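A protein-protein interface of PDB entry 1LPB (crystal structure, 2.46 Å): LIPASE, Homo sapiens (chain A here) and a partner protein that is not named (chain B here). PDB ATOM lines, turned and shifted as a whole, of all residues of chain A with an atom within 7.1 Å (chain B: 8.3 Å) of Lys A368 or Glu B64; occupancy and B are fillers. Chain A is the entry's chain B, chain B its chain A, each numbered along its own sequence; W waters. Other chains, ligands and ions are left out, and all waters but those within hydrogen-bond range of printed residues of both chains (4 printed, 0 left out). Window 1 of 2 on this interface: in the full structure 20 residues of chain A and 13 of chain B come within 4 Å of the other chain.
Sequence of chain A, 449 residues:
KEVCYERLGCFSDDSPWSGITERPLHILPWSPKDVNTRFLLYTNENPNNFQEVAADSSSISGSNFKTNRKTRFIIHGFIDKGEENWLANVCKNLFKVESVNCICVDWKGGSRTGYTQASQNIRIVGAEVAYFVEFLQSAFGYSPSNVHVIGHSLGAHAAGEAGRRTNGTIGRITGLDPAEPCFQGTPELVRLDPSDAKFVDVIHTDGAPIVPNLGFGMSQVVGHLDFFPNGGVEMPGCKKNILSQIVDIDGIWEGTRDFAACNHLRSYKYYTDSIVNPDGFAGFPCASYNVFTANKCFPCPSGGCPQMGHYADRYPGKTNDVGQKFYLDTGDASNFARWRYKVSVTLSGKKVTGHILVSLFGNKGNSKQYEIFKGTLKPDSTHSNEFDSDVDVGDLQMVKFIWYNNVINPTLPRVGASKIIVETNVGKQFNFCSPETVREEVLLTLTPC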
ATOM      1  N   ASP A 332      -8.837  18.379  30.265  1.00  0.00           N
ATOM      2  CA  ASP A 332      -7.895  19.498  30.308  1.00  0.00           C
ATOM      3  C   ASP A 332      -8.621  20.847  30.414  1.00  0.00           C
ATOM      4  O   ASP A 332      -7.989  21.903  30.454  1.00  0.00           O
ATOM      5  CB  ASP A 332      -7.027  19.498  29.055  1.00  0.00           C
ATOM      6  CG  ASP A 332      -7.770  20.016  27.847  1.00  0.00           C
ATOM      7  OD1 ASP A 332      -8.749  19.351  27.449  1.00  0.00           O
ATOM      8  OD2 ASP A 332      -7.411  21.104  27.329  1.00  0.00           O
ATOM      9  N   ARG A 338     -14.522  12.360  32.963  1.00  0.00           N
ATOM     10  CA  ARG A 338     -14.073  11.374  31.980  1.00  0.00           C
ATOM     11  C   ARG A 338     -14.566  10.007  32.437  1.00  0.00           C
ATOM     12  O   ARG A 338     -14.561   9.721  33.645  1.00  0.00           O
ATOM     13  CB  ARG A 338     -12.540  11.266  31.992  1.00  0.00           C
ATOM     14  CG  ARG A 338     -11.752  12.429  31.458  1.00  0.00           C
ATOM     15  CD  ARG A 338     -12.057  12.735  29.996  1.00  0.00           C
ATOM     16  NE  ARG A 338     -12.941  13.877  29.957  1.00  0.00           N
ATOM     17  CZ  ARG A 338     -12.697  15.014  29.323  1.00  0.00           C
ATOM     18  NH1 ARG A 338     -11.644  15.135  28.512  1.00  0.00           N
ATOM     19  NH2 ARG A 338     -13.576  16.001  29.431  1.00  0.00           N
ATOM     20  N   LEU A 357      -8.280   2.780  15.292  1.00  0.00           N
ATOM     21  CA  LEU A 357      -9.204   3.594  16.076  1.00  0.00           C
ATOM     22  C   LEU A 357     -10.558   2.940  16.205  1.00  0.00           C
ATOM     23  O   LEU A 357     -11.016   2.203  15.330  1.00  0.00           O
ATOM     24  CB  LEU A 357      -9.377   4.976  15.445  1.00  0.00           C
ATOM     25  CG  LEU A 357      -8.057   5.670  15.136  1.00  0.00           C
ATOM     26  CD1 LEU A 357      -7.615   5.269  13.748  1.00  0.00           C
ATOM     27  CD2 LEU A 357      -8.215   7.151  15.220  1.00  0.00           C
ATOM     28  N   VAL A 358     -11.232   3.298  17.281  1.00  0.00           N
ATOM     29  CA  VAL A 358     -12.537   2.753  17.604  1.00  0.00           C
ATOM     30  C   VAL A 358     -13.387   3.891  18.202  1.00  0.00           C
ATOM     31  O   VAL A 358     -12.847   4.859  18.745  1.00  0.00           O
ATOM     32  CB  VAL A 358     -12.334   1.570  18.632  1.00  0.00           C
ATOM     33  CG1 VAL A 358     -13.524   1.390  19.506  1.00  0.00           C
ATOM     34  CG2 VAL A 358     -12.016   0.242  17.897  1.00  0.00           C
ATOM     35  N   SER A 359     -14.691   3.866  17.940  1.00  0.00           N
ATOM     36  CA  SER A 359     -15.603   4.842  18.534  1.00  0.00           C
ATOM     37  C   SER A 359     -16.773   4.001  19.069  1.00  0.00           C
ATOM     38  O   SER A 359     -17.089   2.940  18.509  1.00  0.00           O
ATOM     39  CB  SER A 359     -16.041   5.926  17.553  1.00  0.00           C
ATOM     40  OG  SER A 359     -16.357   5.370  16.292  1.00  0.00           O
ATOM     41  N   LEU A 360     -17.350   4.444  20.189  1.00  0.00           N
ATOM     42  CA  LEU A 360     -18.423   3.725  20.853  1.00  0.00           C
ATOM     43  C   LEU A 360     -19.765   4.395  20.671  1.00  0.00           C
ATOM     44  O   LEU A 360     -19.861   5.633  20.688  1.00  0.00           O
ATOM     45  CB  LEU A 360     -18.106   3.582  22.349  1.00  0.00           C
ATOM     46  CG  LEU A 360     -16.625   3.394  22.749  1.00  0.00           C
ATOM     47  CD1 LEU A 360     -16.511   3.250  24.262  1.00  0.00           C
ATOM     48  CD2 LEU A 360     -16.031   2.198  22.071  1.00  0.00           C
ATOM     49  N   ASN A 366     -22.660   8.723  21.421  1.00  0.00           N
ATOM     50  CA  ASN A 366     -21.438   8.165  20.892  1.00  0.00           C
ATOM     51  C   ASN A 366     -20.234   9.016  21.247  1.00  0.00           C
ATOM     52  O   ASN A 366     -20.369  10.115  21.770  1.00  0.00           O
ATOM     53  CB  ASN A 366     -21.559   7.981  19.363  1.00  0.00           C
ATOM     54  CG  ASN A 366     -21.762   9.296  18.595  1.00  0.00           C
ATOM     55  OD1 ASN A 366     -22.866   9.859  18.567  1.00  0.00           O
ATOM     56  ND2 ASN A 366     -20.713   9.757  17.925  1.00  0.00           N
ATOM     57  N   SER A 367     -19.048   8.524  20.966  1.00  0.00           N
ATOM     58  CA  SER A 367     -17.866   9.284  21.303  1.00  0.00           C
ATOM     59  C   SER A 367     -16.980   9.559  20.097  1.00  0.00           C
ATOM     60  O   SER A 367     -17.341   9.229  18.950  1.00  0.00           O
ATOM     61  CB  SER A 367     -17.051   8.474  22.302  1.00  0.00           C
ATOM     62  OG  SER A 367     -16.456   7.353  21.655  1.00  0.00           O
ATOM     63  N   LYS A 368     -15.816  10.150  20.400  1.00  0.00           N
ATOM     64  CA  LYS A 368     -14.720  10.441  19.466  1.00  0.00           C
ATOM     65  C   LYS A 368     -14.075   9.084  19.130  1.00  0.00           C
ATOM     66  O   LYS A 368     -14.376   8.058  19.763  1.00  0.00           O
ATOM     67  CB  LYS A 368     -13.625  11.259  20.169  1.00  0.00           C
ATOM     68  CG  LYS A 368     -14.081  12.531  20.852  1.00  0.00           C
ATOM     69  CD  LYS A 368     -12.949  13.177  21.662  1.00  0.00           C
ATOM     70  CE  LYS A 368     -13.416  14.471  22.363  1.00  0.00           C
ATOM     71  NZ  LYS A 368     -12.502  15.005  23.452  1.00  0.00           N
ATOM     72  N   GLN A 369     -13.198   9.068  18.137  1.00  0.00           N
ATOM     73  CA  GLN A 369     -12.486   7.847  17.775  1.00  0.00           C
ATOM     74  C   GLN A 369     -11.250   7.929  18.660  1.00  0.00           C
ATOM     75  O   GLN A 369     -10.678   9.008  18.815  1.00  0.00           O
ATOM     76  CB  GLN A 369     -12.098   7.863  16.299  1.00  0.00           C
ATOM     77  CG  GLN A 369     -13.280   7.708  15.334  1.00  0.00           C
ATOM     78  CD  GLN A 369     -12.950   8.196  13.914  1.00  0.00           C
ATOM     79  OE1 GLN A 369     -11.849   8.675  13.638  1.00  0.00           O
ATOM     80  NE2 GLN A 369     -13.922   8.100  13.023  1.00  0.00           N
ATOM     81  N   TYR A 370     -10.891   6.819  19.298  1.00  0.00           N
ATOM     82  CA  TYR A 370      -9.752   6.764  20.215  1.00  0.00           C
ATOM     83  C   TYR A 370      -8.740   5.832  19.651  1.00  0.00           C
ATOM     84  O   TYR A 370      -9.092   4.756  19.201  1.00  0.00           O
ATOM     85  CB  TYR A 370     -10.204   6.250  21.591  1.00  0.00           C
ATOM     86  CG  TYR A 370     -10.955   7.306  22.353  1.00  0.00           C
ATOM     87  CD1 TYR A 370     -10.272   8.344  22.966  1.00  0.00           C
ATOM     88  CD2 TYR A 370     -12.358   7.330  22.384  1.00  0.00           C
ATOM     89  CE1 TYR A 370     -10.951   9.386  23.587  1.00  0.00           C
ATOM     90  CE2 TYR A 370     -13.047   8.385  23.000  1.00  0.00           C
ATOM     91  CZ  TYR A 370     -12.320   9.400  23.592  1.00  0.00           C
ATOM     92  OH  TYR A 370     -12.943  10.459  24.191  1.00  0.00           O
ATOM     93  N   PHE A 387      -9.085   3.843  27.826  1.00  0.00           N
ATOM     94  CA  PHE A 387      -9.007   5.250  27.477  1.00  0.00           C
ATOM     95  C   PHE A 387     -10.064   6.013  28.215  1.00  0.00           C
ATOM     96  O   PHE A 387     -11.039   5.401  28.668  1.00  0.00           O
ATOM     97  CB  PHE A 387      -9.108   5.479  25.951  1.00  0.00           C
ATOM     98  CG  PHE A 387     -10.310   4.848  25.306  1.00  0.00           C
ATOM     99  CD1 PHE A 387     -11.563   5.461  25.374  1.00  0.00           C
ATOM    100  CD2 PHE A 387     -10.183   3.664  24.591  1.00  0.00           C
ATOM    101  CE1 PHE A 387     -12.668   4.912  24.737  1.00  0.00           C
ATOM    102  CE2 PHE A 387     -11.294   3.096  23.942  1.00  0.00           C
ATOM    103  CZ  PHE A 387     -12.533   3.719  24.013  1.00  0.00           C
ATOM    104  N   ASP A 388      -9.870   7.326  28.360  1.00  0.00           N
ATOM    105  CA  ASP A 388     -10.834   8.160  29.077  1.00  0.00           C
ATOM    106  C   ASP A 388     -11.714   8.935  28.138  1.00  0.00           C
ATOM    107  O   ASP A 388     -11.296   9.948  27.571  1.00  0.00           O
ATOM    108  CB  ASP A 388     -10.145   9.119  30.043  1.00  0.00           C
ATOM    109  CG  ASP A 388      -9.139   8.416  30.927  1.00  0.00           C
ATOM    110  OD1 ASP A 388      -9.522   7.584  31.774  1.00  0.00           O
ATOM    111  OD2 ASP A 388      -7.939   8.672  30.745  1.00  0.00           O
ATOM    112  N   SER A 389     -12.950   8.472  28.020  1.00  0.00           N
ATOM    113  CA  SER A 389     -13.961   9.078  27.158  1.00  0.00           C
ATOM    114  C   SER A 389     -14.565  10.358  27.789  1.00  0.00           C
ATOM    115  O   SER A 389     -14.739  10.451  29.014  1.00  0.00           O
ATOM    116  CB  SER A 389     -15.057   8.010  26.897  1.00  0.00           C
ATOM    117  OG  SER A 389     -16.073   8.423  25.995  1.00  0.00           O
ATOM    118  N   ASP A 390     -14.848  11.362  26.965  1.00  0.00           N
ATOM    119  CA  ASP A 390     -15.480  12.591  27.457  1.00  0.00           C
ATOM    120  C   ASP A 390     -17.028  12.446  27.560  1.00  0.00           C
ATOM    121  O   ASP A 390     -17.732  13.353  28.005  1.00  0.00           O
ATOM    122  CB  ASP A 390     -15.029  13.844  26.660  1.00  0.00           C
ATOM    123  CG  ASP A 390     -15.625  13.937  25.242  1.00  0.00           C
ATOM    124  OD1 ASP A 390     -15.838  12.934  24.538  1.00  0.00           O
ATOM    125  OD2 ASP A 390     -15.838  15.077  24.811  1.00  0.00           O
ATOM    126  N   VAL A 391     -17.542  11.284  27.160  1.00  0.00           N
ATOM    127  CA  VAL A 391     -18.963  10.979  27.285  1.00  0.00           C
ATOM    128  C   VAL A 391     -19.196   9.576  27.836  1.00  0.00           C
ATOM    129  O   VAL A 391     -18.387   8.661  27.651  1.00  0.00           O
ATOM    130  CB  VAL A 391     -19.720  11.027  25.957  1.00  0.00           C
ATOM    131  CG1 VAL A 391     -19.913  12.430  25.509  1.00  0.00           C
ATOM    132  CG2 VAL A 391     -19.012  10.214  24.928  1.00  0.00           C
ATOM    133  N   ILE A 402     -11.713   1.483  12.573  1.00  0.00           N
ATOM    134  CA  ILE A 402     -11.124   2.279  11.488  1.00  0.00           C
ATOM    135  C   ILE A 402      -9.598   2.342  11.606  1.00  0.00           C
ATOM    136  O   ILE A 402      -9.057   2.456  12.707  1.00  0.00           O
ATOM    137  CB  ILE A 402     -11.739   3.740  11.419  1.00  0.00           C
ATOM    138  CG1 ILE A 402     -11.274   4.440  10.150  1.00  0.00           C
ATOM    139  CG2 ILE A 402     -11.292   4.591  12.611  1.00  0.00           C
ATOM    140  CD1 ILE A 402     -11.974   5.713   9.891  1.00  0.00           C
ATOM    141  N   LEU A 443     -15.060   3.555   7.877  1.00  0.00           N
ATOM    142  CA  LEU A 443     -15.545   2.994   9.136  1.00  0.00           C
ATOM    143  C   LEU A 443     -16.117   1.597   8.914  1.00  0.00           C
ATOM    144  O   LEU A 443     -16.936   1.380   8.008  1.00  0.00           O
ATOM    145  CB  LEU A 443     -16.659   3.835   9.753  1.00  0.00           C
ATOM    146  CG  LEU A 443     -16.443   5.096  10.591  1.00  0.00           C
ATOM    147  CD1 LEU A 443     -15.265   4.928  11.546  1.00  0.00           C
ATOM    148  CD2 LEU A 443     -16.250   6.282   9.677  1.00  0.00           C
ATOM    149  N   GLU B  13      -4.969  21.609  21.864  1.00  0.00           N
ATOM    150  CA  GLU B  13      -6.323  22.116  21.922  1.00  0.00           C
ATOM    151  C   GLU B  13      -6.389  23.201  23.004  1.00  0.00           C
ATOM    152  O   GLU B  13      -5.669  23.129  24.007  1.00  0.00           O
ATOM    153  CB  GLU B  13      -7.291  20.958  22.155  1.00  0.00           C
ATOM    154  CG  GLU B  13      -7.315  19.969  20.977  1.00  0.00           C
ATOM    155  CD  GLU B  13      -6.408  18.741  21.165  1.00  0.00           C
ATOM    156  OE1 GLU B  13      -6.412  18.153  22.280  1.00  0.00           O
ATOM    157  OE2 GLU B  13      -5.718  18.335  20.191  1.00  0.00           O
ATOM    158  N   LEU B  41     -10.865  20.014  18.779  1.00  0.00           N
ATOM    159  CA  LEU B  41     -10.928  18.678  18.173  1.00  0.00           C
ATOM    160  C   LEU B  41     -11.925  18.671  17.018  1.00  0.00           C
ATOM    161  O   LEU B  41     -12.887  19.445  17.026  1.00  0.00           O
ATOM    162  CB  LEU B  41     -11.343  17.626  19.203  1.00  0.00           C
ATOM    163  CG  LEU B  41     -10.390  17.465  20.387  1.00  0.00           C
ATOM    164  CD1 LEU B  41     -11.089  16.734  21.500  1.00  0.00           C
ATOM    165  CD2 LEU B  41      -9.129  16.756  19.968  1.00  0.00           C
ATOM    166  N   LYS B  42     -11.672  17.832  16.013  1.00  0.00           N
ATOM    167  CA  LYS B  42     -12.581  17.726  14.868  1.00  0.00           C
ATOM    168  C   LYS B  42     -13.905  17.111  15.332  1.00  0.00           C
ATOM    169  O   LYS B  42     -13.932  16.325  16.291  1.00  0.00           O
ATOM    170  CB  LYS B  42     -11.973  16.868  13.754  1.00  0.00           C
ATOM    171  CG  LYS B  42     -10.687  17.409  13.172  1.00  0.00           C
ATOM    172  CD  LYS B  42     -10.366  16.705  11.872  1.00  0.00           C
ATOM    173  CE  LYS B  42      -8.872  16.689  11.556  1.00  0.00           C
ATOM    174  NZ  LYS B  42      -8.308  18.033  11.241  1.00  0.00           N
ATOM    175  N   ALA B  43     -14.994  17.447  14.646  1.00  0.00           N
ATOM    176  CA  ALA B  43     -16.322  16.943  15.004  1.00  0.00           C
ATOM    177  C   ALA B  43     -16.456  15.417  14.948  1.00  0.00           C
ATOM    178  O   ALA B  43     -16.037  14.779  13.976  1.00  0.00           O
ATOM    179  CB  ALA B  43     -17.356  17.582  14.138  1.00  0.00           C
ATOM    180  N   ARG B  44     -16.985  14.831  16.024  1.00  0.00           N
ATOM    181  CA  ARG B  44     -17.205  13.388  16.102  1.00  0.00           C
ATOM    182  C   ARG B  44     -18.478  13.094  15.311  1.00  0.00           C
ATOM    183  O   ARG B  44     -19.169  14.012  14.887  1.00  0.00           O
ATOM    184  CB  ARG B  44     -17.346  12.926  17.564  1.00  0.00           C
ATOM    185  CG  ARG B  44     -18.707  13.162  18.227  1.00  0.00           C
ATOM    186  CD  ARG B  44     -18.645  12.885  19.727  1.00  0.00           C
ATOM    187  NE  ARG B  44     -17.602  13.691  20.369  1.00  0.00           N
ATOM    188  CZ  ARG B  44     -17.291  13.658  21.668  1.00  0.00           C
ATOM    189  NH1 ARG B  44     -17.941  12.852  22.503  1.00  0.00           N
ATOM    190  NH2 ARG B  44     -16.314  14.433  22.136  1.00  0.00           N
ATOM    191  N   GLU B  45     -18.786  11.824  15.099  1.00  0.00           N
ATOM    192  CA  GLU B  45     -19.988  11.453  14.352  1.00  0.00           C
ATOM    193  C   GLU B  45     -21.266  12.013  14.982  1.00  0.00           C
ATOM    194  O   GLU B  45     -21.375  12.103  16.204  1.00  0.00           O
ATOM    195  CB  GLU B  45     -20.087   9.919  14.233  1.00  0.00           C
ATOM    196  CG  GLU B  45     -21.197   9.400  13.323  1.00  0.00           C
ATOM    197  CD  GLU B  45     -21.010   7.937  12.948  1.00  0.00           C
ATOM    198  OE1 GLU B  45     -19.860   7.488  12.891  1.00  0.00           O
ATOM    199  OE2 GLU B  45     -22.013   7.226  12.724  1.00  0.00           O
ATOM    200  N   ASN B  46     -22.195  12.407  14.113  1.00  0.00           N
ATOM    201  CA  ASN B  46     -23.520  12.938  14.454  1.00  0.00           C
ATOM    202  C   ASN B  46     -23.623  14.303  15.071  1.00  0.00           C
ATOM    203  O   ASN B  46     -24.731  14.695  15.495  1.00  0.00           O
ATOM    204  CB  ASN B  46     -24.296  11.973  15.324  1.00  0.00           C
ATOM    205  CG  ASN B  46     -24.466  10.661  14.678  1.00  0.00           C
ATOM    206  OD1 ASN B  46     -24.956  10.583  13.556  1.00  0.00           O
ATOM    207  ND2 ASN B  46     -24.010   9.609  15.339  1.00  0.00           N
ATOM    208  N   SER B  47     -22.500  15.026  15.131  1.00  0.00           N
ATOM    209  CA  SER B  47     -22.499  16.373  15.683  1.00  0.00           C
ATOM    210  C   SER B  47     -22.217  17.383  14.586  1.00  0.00           C
ATOM    211  O   SER B  47     -21.884  17.021  13.456  1.00  0.00           O
ATOM    212  CB  SER B  47     -21.488  16.487  16.801  1.00  0.00           C
ATOM    213  OG  SER B  47     -20.202  16.172  16.315  1.00  0.00           O
ATOM    214  N   CYS B  49     -20.588  20.183  12.141  1.00  0.00           N
ATOM    215  CA  CYS B  49     -19.305  20.368  11.496  1.00  0.00           C
ATOM    216  C   CYS B  49     -19.347  21.491  10.469  1.00  0.00           C
ATOM    217  O   CYS B  49     -20.338  22.220  10.345  1.00  0.00           O
ATOM    218  CB  CYS B  49     -18.910  19.063  10.797  1.00  0.00           C
ATOM    219  SG  CYS B  49     -20.288  18.322   9.866  1.00  0.00           S
ATOM    220  N   CYS B  61     -15.836  22.611  13.444  1.00  0.00           N
ATOM    221  CA  CYS B  61     -14.746  21.841  12.903  1.00  0.00           C
ATOM    222  C   CYS B  61     -15.164  20.780  11.902  1.00  0.00           C
ATOM    223  O   CYS B  61     -16.303  20.308  11.916  1.00  0.00           O
ATOM    224  CB  CYS B  61     -14.020  21.109  14.034  1.00  0.00           C
ATOM    225  SG  CYS B  61     -13.005  22.084  15.173  1.00  0.00           S
ATOM    226  N   PRO B  62     -14.241  20.413  10.994  1.00  0.00           N
ATOM    227  CA  PRO B  62     -14.527  19.380  10.011  1.00  0.00           C
ATOM    228  C   PRO B  62     -14.618  18.064  10.809  1.00  0.00           C
ATOM    229  O   PRO B  62     -14.166  17.981  11.968  1.00  0.00           O
ATOM    230  CB  PRO B  62     -13.272  19.412   9.128  1.00  0.00           C
ATOM    231  CG  PRO B  62     -12.183  19.935  10.058  1.00  0.00           C
ATOM    232  CD  PRO B  62     -12.924  21.030  10.740  1.00  0.00           C
ATOM    233  N   CYS B  63     -15.190  17.036  10.199  1.00  0.00           N
ATOM    234  CA  CYS B  63     -15.348  15.739  10.858  1.00  0.00           C
ATOM    235  C   CYS B  63     -14.052  14.960  10.953  1.00  0.00           C
ATOM    236  O   CYS B  63     -13.047  15.342  10.362  1.00  0.00           O
ATOM    237  CB  CYS B  63     -16.366  14.890  10.110  1.00  0.00           C
ATOM    238  SG  CYS B  63     -17.956  15.723   9.850  1.00  0.00           S
ATOM    239  N   GLU B  64     -14.083  13.897  11.748  1.00  0.00           N
ATOM    240  CA  GLU B  64     -12.940  13.013  11.925  1.00  0.00           C
ATOM    241  C   GLU B  64     -12.816  12.080  10.700  1.00  0.00           C
ATOM    242  O   GLU B  64     -13.641  12.105   9.785  1.00  0.00           O
ATOM    243  CB  GLU B  64     -13.129  12.159  13.175  1.00  0.00           C
ATOM    244  CG  GLU B  64     -13.267  12.913  14.482  1.00  0.00           C
ATOM    245  CD  GLU B  64     -13.763  11.995  15.571  1.00  0.00           C
ATOM    246  OE1 GLU B  64     -14.838  11.415  15.382  1.00  0.00           O
ATOM    247  OE2 GLU B  64     -13.080  11.822  16.592  1.00  0.00           O
ATOM    248  N   ARG B  65     -11.850  11.184  10.724  1.00  0.00           N
ATOM    249  CA  ARG B  65     -11.657  10.315   9.584  1.00  0.00           C
ATOM    250  C   ARG B  65     -12.816   9.406   9.253  1.00  0.00           C
ATOM    251  O   ARG B  65     -13.538   8.922  10.147  1.00  0.00           O
ATOM    252  CB  ARG B  65     -10.368   9.508   9.706  1.00  0.00           C
ATOM    253  CG  ARG B  65      -9.766   9.535  11.074  1.00  0.00           C
ATOM    254  CD  ARG B  65      -8.456   8.835  11.064  1.00  0.00           C
ATOM    255  NE  ARG B  65      -7.545   9.520  10.168  1.00  0.00           N
ATOM    256  CZ  ARG B  65      -6.576  10.322  10.573  1.00  0.00           C
ATOM    257  NH1 ARG B  65      -6.376  10.521  11.875  1.00  0.00           N
ATOM    258  NH2 ARG B  65      -5.799  10.901   9.662  1.00  0.00           N
ATOM    259  N   GLY B  66     -12.991   9.222   7.943  1.00  0.00           N
ATOM    260  CA  GLY B  66     -14.026   8.365   7.394  1.00  0.00           C
ATOM    261  C   GLY B  66     -15.405   8.964   7.482  1.00  0.00           C
ATOM    262  O   GLY B  66     -16.401   8.334   7.112  1.00  0.00           O
ATOM    263  N   LEU B  67     -15.464  10.209   7.922  1.00  0.00           N
ATOM    264  CA  LEU B  67     -16.735  10.862   8.079  1.00  0.00           C
ATOM    265  C   LEU B  67     -16.979  11.998   7.089  1.00  0.00           C
ATOM    266  O   LEU B  67     -16.061  12.729   6.707  1.00  0.00           O
ATOM    267  CB  LEU B  67     -16.812  11.368   9.504  1.00  0.00           C
ATOM    268  CG  LEU B  67     -17.665  10.690  10.563  1.00  0.00           C
ATOM    269  CD1 LEU B  67     -17.690   9.201  10.422  1.00  0.00           C
ATOM    270  CD2 LEU B  67     -17.112  11.126  11.898  1.00  0.00           C
ATOM    271  N   THR B  68     -18.234  12.161   6.699  1.00  0.00           N
ATOM    272  CA  THR B  68     -18.628  13.210   5.776  1.00  0.00           C
ATOM    273  C   THR B  68     -19.508  14.231   6.462  1.00  0.00           C
ATOM    274  O   THR B  68     -20.503  13.880   7.096  1.00  0.00           O
ATOM    275  CB  THR B  68     -19.481  12.674   4.619  1.00  0.00           C
ATOM    276  OG1 THR B  68     -18.821  11.585   3.962  1.00  0.00           O
ATOM    277  CG2 THR B  68     -19.728  13.793   3.629  1.00  0.00           C
ATOM    278  N   CYS B  69     -19.191  15.500   6.278  1.00  0.00           N
ATOM    279  CA  CYS B  69     -20.009  16.538   6.860  1.00  0.00           C
ATOM    280  C   CYS B  69     -21.144  16.855   5.887  1.00  0.00           C
ATOM    281  O   CYS B  69     -20.966  17.597   4.929  1.00  0.00           O
ATOM    282  CB  CYS B  69     -19.180  17.791   7.128  1.00  0.00           C
ATOM    283  SG  CYS B  69     -20.153  19.062   7.983  1.00  0.00           S
ATOM    284  N   CYS B  87     -21.788  15.443  10.951  1.00  0.00           N
ATOM    285  CA  CYS B  87     -20.900  14.338  10.614  1.00  0.00           C
ATOM    286  C   CYS B  87     -21.603  12.996  10.436  1.00  0.00           C
ATOM    287  O   CYS B  87     -22.112  12.433  11.386  1.00  0.00           O
ATOM    288  CB  CYS B  87     -19.819  14.221  11.675  1.00  0.00           C
ATOM    289  SG  CYS B  87     -18.776  15.702  11.700  1.00  0.00           S
ATOM    290  N   HIS B  88     -21.596  12.462   9.223  1.00  0.00           N
ATOM    291  CA  HIS B  88     -22.241  11.189   8.956  1.00  0.00           C
ATOM    292  C   HIS B  88     -21.345  10.131   8.366  1.00  0.00           C
ATOM    293  O   HIS B  88     -20.432  10.444   7.624  1.00  0.00           O
ATOM    294  CB  HIS B  88     -23.447  11.391   8.050  1.00  0.00           C
ATOM    295  CG  HIS B  88     -24.638  11.909   8.776  1.00  0.00           C
ATOM    296  ND1 HIS B  88     -25.524  12.806   8.221  1.00  0.00           N
ATOM    297  CD2 HIS B  88     -25.052  11.705  10.050  1.00  0.00           C
ATOM    298  CE1 HIS B  88     -26.430  13.134   9.125  1.00  0.00           C
ATOM    299  NE2 HIS B  88     -26.165  12.482  10.243  1.00  0.00           N
HETATM  300  O   HOH W   1      -4.869  21.169  26.031  1.00  0.00           O
HETATM  301  O   HOH W   2     -15.488  10.730  23.333  1.00  0.00           O
HETATM  302  O   HOH W   3     -16.975   9.937  16.011  1.00  0.00           O
HETATM  303  O   HOH W   4     -16.491   5.414   6.596  1.00  0.00           O
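Ser A367 touches just one residue of chain B: Arg B44.
Of the printed residues of chain A, Arg B44 touches Asn A366, Ser A367, Lys A368, Asp A390 and Val A391.
Printed residues of chain A within 4 Å of Arg B65: Gln A369 (3.0 Å), Ile A402 (3.6 Å) and Leu A443 (3.8 Å).
Printed residues of chain A within 4 Å of Leu B67: Leu A443 (3.3 Å).
His B88 touches none of the printed residues of chain A.
The nearest residue of chain A that does not touch Glu B64 is Ser A367 (4.9 Å).
Printed residues of chain B that touch a printed residue of chain A: Leu B41, Arg B44, Glu B45, Asn B46, Glu B64, Arg B65, Gly B66 and Leu B67.
Hydrophobic or aromatic side chains of chain B within 4 Å of the printed part of chain A: Leu B41 and Leu B67.
Along chain B the printed residues that touch a printed residue of chain A span positions 41 to 67.
Printed residues of chain A that touch a printed residue of chain B: Asn A366, Ser A367, Lys A368, Gln A369, Asp A390, Val A391, Ile A402 and Leu A443.
N of Glu B64 sits at hydrogen-bond distance from O of Ala B43 (3.1 Å).
OG of Ser B47 is in hydrogen-bond range of O of Arg B44, 2.8 Å away.
The backbone carbonyl oxygen (O) of Ile A402 sits at hydrogen-bond distance from the backbone NH (N) of Leu A357 (2.7 Å).
OH of Tyr A370 sits at hydrogen-bond distance from N of Asp A390, 3.5 Å away.
The side-chain sulfur of Cys B63 forms a disulfide with the side-chain sulfur of Cys B87, at 2.0 Å.
Among the printed residues, merely in contact across the chains: Lys A368 with Arg B44, Lys A368 with Leu B41, Leu A443 with Gly B66, Leu A443 with Leu B67, Ile A402 with Arg B65, Lys A368 with Glu B64, Val A391 with Arg B44, Asn A366 with Arg B44, Ser A367 with Arg B44 and Leu A443 with Arg B65.
Water W4 lies within hydrogen-bond range of the backbone NH of Leu A443 (2.7 Å) and the backbone carbonyl oxygen of Gly B66 (3.0 Å).
Water W1 lies within hydrogen-bond range of the side-chain carboxylate of Asp A332 and the backbone carbonyl oxygen of Glu B13.
The guanidinium group (NH2) of Arg B44 lies within salt-bridge range of the side-chain carboxylate (OD2) of Asp A390 (2.8 Å).
O of Glu B45 is in hydrogen-bond range of ND2 of Asn A366, at 3.0 Å.
The side-chain amide nitrogen (ND2) of Asn B46 lies within hydrogen-bond range of the side-chain amide oxygen (OD1) of Asn A366, at 3.4 Å.
N of Gln A369 sits at hydrogen-bond distance from OE2 of Glu B64 (3.2 Å).
O of Arg B65 is in hydrogen-bond range of NE2 of Gln A369 (3.0 Å).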
